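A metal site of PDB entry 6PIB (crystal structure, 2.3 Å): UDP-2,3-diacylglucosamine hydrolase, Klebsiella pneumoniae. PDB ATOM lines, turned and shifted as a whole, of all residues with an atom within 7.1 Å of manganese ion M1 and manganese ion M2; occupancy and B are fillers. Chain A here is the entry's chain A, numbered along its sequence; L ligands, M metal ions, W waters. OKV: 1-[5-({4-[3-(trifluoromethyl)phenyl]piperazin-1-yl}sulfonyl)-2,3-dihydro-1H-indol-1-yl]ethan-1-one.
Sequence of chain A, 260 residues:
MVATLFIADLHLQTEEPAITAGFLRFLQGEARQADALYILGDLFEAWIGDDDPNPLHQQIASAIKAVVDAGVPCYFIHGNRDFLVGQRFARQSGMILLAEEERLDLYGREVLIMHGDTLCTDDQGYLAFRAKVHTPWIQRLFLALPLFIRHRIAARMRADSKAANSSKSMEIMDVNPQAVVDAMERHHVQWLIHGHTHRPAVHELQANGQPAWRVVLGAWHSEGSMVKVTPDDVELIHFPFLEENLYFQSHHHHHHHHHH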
ATOM      1  N   ALA A   8      12.524  -7.681 -31.304  1.00  0.00           N
ATOM      2  CA  ALA A   8      12.982  -7.564 -29.929  1.00  0.00           C
ATOM      3  C   ALA A   8      14.352  -6.890 -29.935  1.00  0.00           C
ATOM      4  O   ALA A   8      15.008  -6.778 -30.972  1.00  0.00           O
ATOM      5  CB  ALA A   8      13.064  -8.922 -29.226  1.00  0.00           C
ATOM      6  N   ASP A   9      14.763  -6.424 -28.747  1.00  0.00           N
ATOM      7  CA  ASP A   9      16.108  -5.902 -28.510  1.00  0.00           C
ATOM      8  C   ASP A   9      16.425  -4.726 -29.429  1.00  0.00           C
ATOM      9  O   ASP A   9      17.474  -4.674 -30.076  1.00  0.00           O
ATOM     10  CB  ASP A   9      17.151  -7.009 -28.648  1.00  0.00           C
ATOM     11  CG  ASP A   9      16.949  -8.119 -27.634  1.00  0.00           C
ATOM     12  OD1 ASP A   9      17.045  -7.841 -26.419  1.00  0.00           O
ATOM     13  OD2 ASP A   9      16.698  -9.272 -28.051  1.00  0.00           O
ATOM     14  N   LEU A  10      15.500  -3.769 -29.480  1.00  0.00           N
ATOM     15  CA  LEU A  10      15.767  -2.544 -30.218  1.00  0.00           C
ATOM     16  C   LEU A  10      16.609  -1.563 -29.399  1.00  0.00           C
ATOM     17  O   LEU A  10      17.394  -0.799 -29.983  1.00  0.00           O
ATOM     18  CB  LEU A  10      14.456  -1.881 -30.641  1.00  0.00           C
ATOM     19  CG  LEU A  10      13.770  -2.479 -31.868  1.00  0.00           C
ATOM     20  CD1 LEU A  10      12.955  -3.710 -31.499  1.00  0.00           C
ATOM     21  CD2 LEU A  10      12.899  -1.431 -32.533  1.00  0.00           C
ATOM     22  N   HIS A  11      16.456  -1.583 -28.076  1.00  0.00           N
ATOM     23  CA  HIS A  11      17.221  -0.725 -27.179  1.00  0.00           C
ATOM     24  C   HIS A  11      17.122   0.737 -27.588  1.00  0.00           C
ATOM     25  O   HIS A  11      18.116   1.464 -27.671  1.00  0.00           O
ATOM     26  CB  HIS A  11      18.684  -1.181 -27.113  1.00  0.00           C
ATOM     27  CG  HIS A  11      18.873  -2.516 -26.465  1.00  0.00           C
ATOM     28  ND1 HIS A  11      19.029  -2.665 -25.100  1.00  0.00           N
ATOM     29  CD2 HIS A  11      18.918  -3.766 -26.990  1.00  0.00           C
ATOM     30  CE1 HIS A  11      19.173  -3.949 -24.810  1.00  0.00           C
ATOM     31  NE2 HIS A  11      19.100  -4.633 -25.943  1.00  0.00           N
ATOM     32  N   LEU A  40       9.271  -8.677 -28.283  1.00  0.00           N
ATOM     33  CA  LEU A  40       9.687  -9.604 -27.238  1.00  0.00           C
ATOM     34  C   LEU A  40      10.763  -9.014 -26.321  1.00  0.00           C
ATOM     35  O   LEU A  40      11.815  -9.620 -26.105  1.00  0.00           O
ATOM     36  CB  LEU A  40      10.166 -10.910 -27.859  1.00  0.00           C
ATOM     37  CG  LEU A  40       9.220 -11.576 -28.857  1.00  0.00           C
ATOM     38  CD1 LEU A  40       9.773 -12.918 -29.314  1.00  0.00           C
ATOM     39  CD2 LEU A  40       7.831 -11.746 -28.258  1.00  0.00           C
ATOM     40  N   GLY A  41      10.504  -7.832 -25.777  1.00  0.00           N
ATOM     41  CA  GLY A  41      11.359  -7.281 -24.752  1.00  0.00           C
ATOM     42  C   GLY A  41      12.460  -6.385 -25.304  1.00  0.00           C
ATOM     43  O   GLY A  41      12.835  -6.453 -26.467  1.00  0.00           O
ATOM     44  N   ASP A  42      12.982  -5.542 -24.405  1.00  0.00           N
ATOM     45  CA  ASP A  42      14.070  -4.621 -24.709  1.00  0.00           C
ATOM     46  C   ASP A  42      13.721  -3.701 -25.881  1.00  0.00           C
ATOM     47  O   ASP A  42      14.561  -3.404 -26.730  1.00  0.00           O
ATOM     48  CB  ASP A  42      15.374  -5.381 -24.987  1.00  0.00           C
ATOM     49  CG  ASP A  42      15.998  -5.935 -23.721  1.00  0.00           C
ATOM     50  OD1 ASP A  42      15.384  -5.767 -22.640  1.00  0.00           O
ATOM     51  OD2 ASP A  42      17.085  -6.548 -23.804  1.00  0.00           O
ATOM     52  N   GLU A  45      16.051   0.979 -24.119  1.00  0.00           N
ATOM     53  CA  GLU A  45      17.288   0.713 -23.396  1.00  0.00           C
ATOM     54  C   GLU A  45      17.087   0.811 -21.889  1.00  0.00           C
ATOM     55  O   GLU A  45      17.768   0.129 -21.123  1.00  0.00           O
ATOM     56  CB  GLU A  45      18.382   1.667 -23.865  1.00  0.00           C
ATOM     57  CG  GLU A  45      19.662   1.654 -23.045  1.00  0.00           C
ATOM     58  CD  GLU A  45      20.414   0.335 -23.133  1.00  0.00           C
ATOM     59  OE1 GLU A  45      20.171  -0.428 -24.092  1.00  0.00           O
ATOM     60  OE2 GLU A  45      21.247   0.062 -22.243  1.00  0.00           O
ATOM     61  N   GLY A  79      11.273  -7.080 -21.290  1.00  0.00           N
ATOM     62  CA  GLY A  79      12.657  -7.498 -21.331  1.00  0.00           C
ATOM     63  C   GLY A  79      13.368  -7.207 -20.024  1.00  0.00           C
ATOM     64  O   GLY A  79      12.775  -6.768 -19.044  1.00  0.00           O
ATOM     65  N   ASN A  80      14.675  -7.462 -20.034  1.00  0.00           N
ATOM     66  CA  ASN A  80      15.482  -7.172 -18.848  1.00  0.00           C
ATOM     67  C   ASN A  80      15.762  -5.688 -18.680  1.00  0.00           C
ATOM     68  O   ASN A  80      16.082  -5.255 -17.574  1.00  0.00           O
ATOM     69  CB  ASN A  80      16.804  -7.946 -18.906  1.00  0.00           C
ATOM     70  CG  ASN A  80      17.606  -7.654 -20.151  1.00  0.00           C
ATOM     71  OD1 ASN A  80      17.309  -8.176 -21.228  1.00  0.00           O
ATOM     72  ND2 ASN A  80      18.628  -6.819 -20.021  1.00  0.00           N
ATOM     73  N   ARG A  81      15.626  -4.903 -19.742  1.00  0.00           N
ATOM     74  CA  ARG A  81      15.869  -3.458 -19.674  1.00  0.00           C
ATOM     75  C   ARG A  81      14.609  -2.673 -19.347  1.00  0.00           C
ATOM     76  O   ARG A  81      14.662  -1.706 -18.591  1.00  0.00           O
ATOM     77  CB  ARG A  81      16.466  -2.957 -20.991  1.00  0.00           C
ATOM     78  CG  ARG A  81      17.698  -3.721 -21.457  1.00  0.00           C
ATOM     79  CD  ARG A  81      18.867  -3.523 -20.512  1.00  0.00           C
ATOM     80  NE  ARG A  81      19.130  -2.106 -20.262  1.00  0.00           N
ATOM     81  CZ  ARG A  81      20.209  -1.650 -19.632  1.00  0.00           C
ATOM     82  NH1 ARG A  81      21.125  -2.496 -19.184  1.00  0.00           N
ATOM     83  NH2 ARG A  81      20.372  -0.347 -19.449  1.00  0.00           N
ATOM     84  N   HIS A 115      11.224 -13.390 -23.711  1.00  0.00           N
ATOM     85  CA  HIS A 115      12.347 -12.506 -23.973  1.00  0.00           C
ATOM     86  C   HIS A 115      13.648 -13.292 -24.116  1.00  0.00           C
ATOM     87  O   HIS A 115      14.471 -12.976 -24.986  1.00  0.00           O
ATOM     88  CB  HIS A 115      12.489 -11.453 -22.881  1.00  0.00           C
ATOM     89  CG  HIS A 115      13.632 -10.514 -23.109  1.00  0.00           C
ATOM     90  ND1 HIS A 115      13.725  -9.701 -24.217  1.00  0.00           N
ATOM     91  CD2 HIS A 115      14.749 -10.274 -22.374  1.00  0.00           C
ATOM     92  CE1 HIS A 115      14.841  -8.993 -24.154  1.00  0.00           C
ATOM     93  NE2 HIS A 115      15.477  -9.324 -23.041  1.00  0.00           N
ATOM     94  N   GLY A 116      13.844 -14.314 -23.283  1.00  0.00           N
ATOM     95  CA  GLY A 116      15.004 -15.174 -23.356  1.00  0.00           C
ATOM     96  C   GLY A 116      15.973 -15.015 -22.211  1.00  0.00           C
ATOM     97  O   GLY A 116      16.849 -15.879 -22.031  1.00  0.00           O
ATOM     98  N   ASP A 117      15.863 -13.940 -21.423  1.00  0.00           N
ATOM     99  CA  ASP A 117      16.804 -13.725 -20.333  1.00  0.00           C
ATOM    100  C   ASP A 117      16.658 -14.785 -19.242  1.00  0.00           C
ATOM    101  O   ASP A 117      17.647 -15.136 -18.591  1.00  0.00           O
ATOM    102  CB  ASP A 117      16.622 -12.323 -19.750  1.00  0.00           C
ATOM    103  CG  ASP A 117      15.246 -12.130 -19.129  1.00  0.00           C
ATOM    104  OD1 ASP A 117      14.241 -12.354 -19.835  1.00  0.00           O
ATOM    105  OD2 ASP A 117      15.176 -11.740 -17.945  1.00  0.00           O
ATOM    106  N   TYR A 126      23.348 -12.142 -12.848  1.00  0.00           N
ATOM    107  CA  TYR A 126      22.145 -11.539 -13.406  1.00  0.00           C
ATOM    108  C   TYR A 126      20.889 -12.093 -12.756  1.00  0.00           C
ATOM    109  O   TYR A 126      19.920 -11.359 -12.529  1.00  0.00           O
ATOM    110  CB  TYR A 126      22.079 -11.732 -14.917  1.00  0.00           C
ATOM    111  CG  TYR A 126      20.721 -11.418 -15.495  1.00  0.00           C
ATOM    112  CD1 TYR A 126      20.282 -10.105 -15.612  1.00  0.00           C
ATOM    113  CD2 TYR A 126      19.853 -12.428 -15.899  1.00  0.00           C
ATOM    114  CE1 TYR A 126      19.026  -9.803 -16.127  1.00  0.00           C
ATOM    115  CE2 TYR A 126      18.611 -12.144 -16.417  1.00  0.00           C
ATOM    116  CZ  TYR A 126      18.201 -10.826 -16.530  1.00  0.00           C
ATOM    117  OH  TYR A 126      16.959 -10.543 -17.048  1.00  0.00           O
ATOM    118  N   GLY A 195      14.658 -13.445 -27.772  1.00  0.00           N
ATOM    119  CA  GLY A 195      15.760 -12.562 -28.126  1.00  0.00           C
ATOM    120  C   GLY A 195      16.823 -12.513 -27.048  1.00  0.00           C
ATOM    121  O   GLY A 195      17.413 -13.544 -26.692  1.00  0.00           O
ATOM    122  N   HIS A 196      17.097 -11.308 -26.536  1.00  0.00           N
ATOM    123  CA  HIS A 196      18.007 -11.071 -25.418  1.00  0.00           C
ATOM    124  C   HIS A 196      19.465 -11.364 -25.751  1.00  0.00           C
ATOM    125  O   HIS A 196      20.335 -10.526 -25.491  1.00  0.00           O
ATOM    126  CB  HIS A 196      17.588 -11.897 -24.190  1.00  0.00           C
ATOM    127  CG  HIS A 196      18.459 -11.686 -22.990  1.00  0.00           C
ATOM    128  ND1 HIS A 196      18.463 -10.519 -22.267  1.00  0.00           N
ATOM    129  CD2 HIS A 196      19.362 -12.500 -22.393  1.00  0.00           C
ATOM    130  CE1 HIS A 196      19.323 -10.619 -21.275  1.00  0.00           C
ATOM    131  NE2 HIS A 196      19.884 -11.811 -21.326  1.00  0.00           N
ATOM    132  N   THR A 197      19.747 -12.533 -26.330  1.00  0.00           N
ATOM    133  CA  THR A 197      21.126 -12.952 -26.548  1.00  0.00           C
ATOM    134  C   THR A 197      21.799 -12.254 -27.727  1.00  0.00           C
ATOM    135  O   THR A 197      23.024 -12.332 -27.846  1.00  0.00           O
ATOM    136  CB  THR A 197      21.190 -14.464 -26.757  1.00  0.00           C
ATOM    137  OG1 THR A 197      20.408 -14.820 -27.905  1.00  0.00           O
ATOM    138  CG2 THR A 197      20.650 -15.199 -25.541  1.00  0.00           C
ATOM    139  N   HIS A 198      21.038 -11.580 -28.593  1.00  0.00           N
ATOM    140  CA  HIS A 198      21.585 -10.816 -29.721  1.00  0.00           C
ATOM    141  C   HIS A 198      22.343 -11.706 -30.708  1.00  0.00           C
ATOM    142  O   HIS A 198      23.304 -11.270 -31.343  1.00  0.00           O
ATOM    143  CB  HIS A 198      22.481  -9.678 -29.247  1.00  0.00           C
ATOM    144  CG  HIS A 198      21.770  -8.622 -28.455  1.00  0.00           C
ATOM    145  ND1 HIS A 198      22.342  -7.411 -28.152  1.00  0.00           N
ATOM    146  CD2 HIS A 198      20.528  -8.609 -27.911  1.00  0.00           C
ATOM    147  CE1 HIS A 198      21.487  -6.692 -27.447  1.00  0.00           C
ATOM    148  NE2 HIS A 198      20.375  -7.396 -27.287  1.00  0.00           N
ATOM    149  N   ALA A 219      19.487  -8.195 -32.379  1.00  0.00           N
ATOM    150  CA  ALA A 219      19.355  -6.836 -31.885  1.00  0.00           C
ATOM    151  C   ALA A 219      19.468  -5.841 -33.037  1.00  0.00           C
ATOM    152  O   ALA A 219      20.102  -6.105 -34.061  1.00  0.00           O
ATOM    153  CB  ALA A 219      20.434  -6.542 -30.842  1.00  0.00           C
HETATM  154  C13 OKV L   1      17.586  -1.961 -16.536  1.00  0.00           C
HETATM  155  C15 OKV L   1      19.577  -3.260 -16.139  1.00  0.00           C
HETATM  156  C17 OKV L   1      19.546  -0.913 -15.576  1.00  0.00           C
HETATM  157  C21 OKV L   1      20.275  -5.767 -16.558  1.00  0.00           C
HETATM  158  C24 OKV L   1      15.579  -0.409  -9.658  1.00  0.00           C
HETATM  159  C26 OKV L   1      13.789  -1.416  -8.433  1.00  0.00           C
HETATM  160  C28 OKV L   1      15.797  -0.580  -7.158  1.00  0.00           C
HETATM  161  C01 OKV L   1      13.646  -1.220 -10.819  1.00  0.00           C
HETATM  162  C02 OKV L   1      14.882  -0.615 -10.842  1.00  0.00           C
HETATM  163  C04 OKV L   1      16.608   0.717 -12.033  1.00  0.00           C
HETATM  164  C05 OKV L   1      17.368   0.668 -13.355  1.00  0.00           C
HETATM  165  C07 OKV L   1      15.345  -0.024 -14.515  1.00  0.00           C
HETATM  166  C08 OKV L   1      14.554   0.027 -13.213  1.00  0.00           C
HETATM  167  C12 OKV L   1      18.224  -0.822 -16.020  1.00  0.00           C
HETATM  168  C14 OKV L   1      18.253  -3.174 -16.592  1.00  0.00           C
HETATM  169  C16 OKV L   1      20.226  -2.144 -15.634  1.00  0.00           C
HETATM  170  C18 OKV L   1      21.644  -2.503 -15.217  1.00  0.00           C
HETATM  171  C19 OKV L   1      21.773  -3.974 -15.474  1.00  0.00           C
HETATM  172  C23 OKV L   1      21.383  -6.805 -16.416  1.00  0.00           C
HETATM  173  C25 OKV L   1      15.032  -0.806  -8.462  1.00  0.00           C
HETATM  174  C27 OKV L   1      13.092  -1.635  -9.610  1.00  0.00           C
HETATM  175  F29 OKV L   1      16.768  -1.489  -7.049  1.00  0.00           F
HETATM  176  F30 OKV L   1      14.969  -0.685  -6.121  1.00  0.00           F
HETATM  177  F31 OKV L   1      16.337   0.640  -7.165  1.00  0.00           F
HETATM  178  N03 OKV L   1      15.450  -0.201 -12.053  1.00  0.00           N
HETATM  179  N06 OKV L   1      16.483   0.888 -14.489  1.00  0.00           N
HETATM  180  N20 OKV L   1      20.525  -4.414 -16.087  1.00  0.00           N
HETATM  181  O10 OKV L   1      16.391   0.809 -17.056  1.00  0.00           O
HETATM  182  O11 OKV L   1      18.299   1.857 -16.063  1.00  0.00           O
HETATM  183  O22 OKV L   1      19.236  -6.048 -17.044  1.00  0.00           O
HETATM  184  S09 OKV L   1      17.341   0.751 -15.951  1.00  0.00           S
HETATM  185 MN    MN M   1      18.633  -6.877 -25.976  1.00  0.00          MN
HETATM  186 MN    MN M   2      17.582  -8.512 -23.076  1.00  0.00          MN
HETATM  187  O   HOH W   1      19.273  -7.911 -24.221  1.00  0.00           O
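Manganese ion M2 is bound by OD1 of Asn 80 (1.9 Å).
Water W1 is bound to manganese ion M2 (2.1 Å).
Manganese ion M2 is bound by the side-chain carboxylate (OD2) of Asp 42 (2.2 Å).
A ring nitrogen (NE2) of His 115 is bound to manganese ion M2.
A ring nitrogen (ND1) of His 196 is bound to manganese ion M2 (2.3 Å).
N of His 196 is in hydrogen-bond range of OD2 of Asp 9.
The backbone NH of Asp 9 sits at hydrogen-bond distance from the backbone carbonyl oxygen of Gly 41 (3.0 Å).
OD1 of Asp 42 sits at hydrogen-bond distance from N of Arg 81, at 3.0 Å.
The backbone carbonyl oxygen of Asp 42 lies within hydrogen-bond range of the backbone NH of Leu 10 (2.9 Å).
O of His 115 lies within hydrogen-bond range of N of Gly 195 (2.8 Å).
O of Leu 40 lies within hydrogen-bond range of ND1 of His 115 (2.7 Å).
ND1 of His 11 lies within hydrogen-bond range of OE1 of Glu 45 (2.7 Å).
Within 4 Å of manganese ion M1: Asp 9, His 11, Asp 42 and His 198.
Within 4 Å of manganese ion M2: Asp 9, Asp 42, Asn 80, His 115 and His 196.
The nearest printed residue that does not touch manganese ion M2 is His 11 (5.1 Å).
Manganese ion M1 is bound by the side-chain carboxylate of Asp 9, water W1, a ring nitrogen (NE2) of His 198, a ring nitrogen (NE2) of His 11 and the side-chain carboxylate of Asp 42.
Manganese ion M1 has five donor atoms within binding distance.
An oxygen (O22) of the ligand is in hydrogen-bond range of the side-chain amide nitrogen (ND2) of Asn 80 (3.1 Å).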
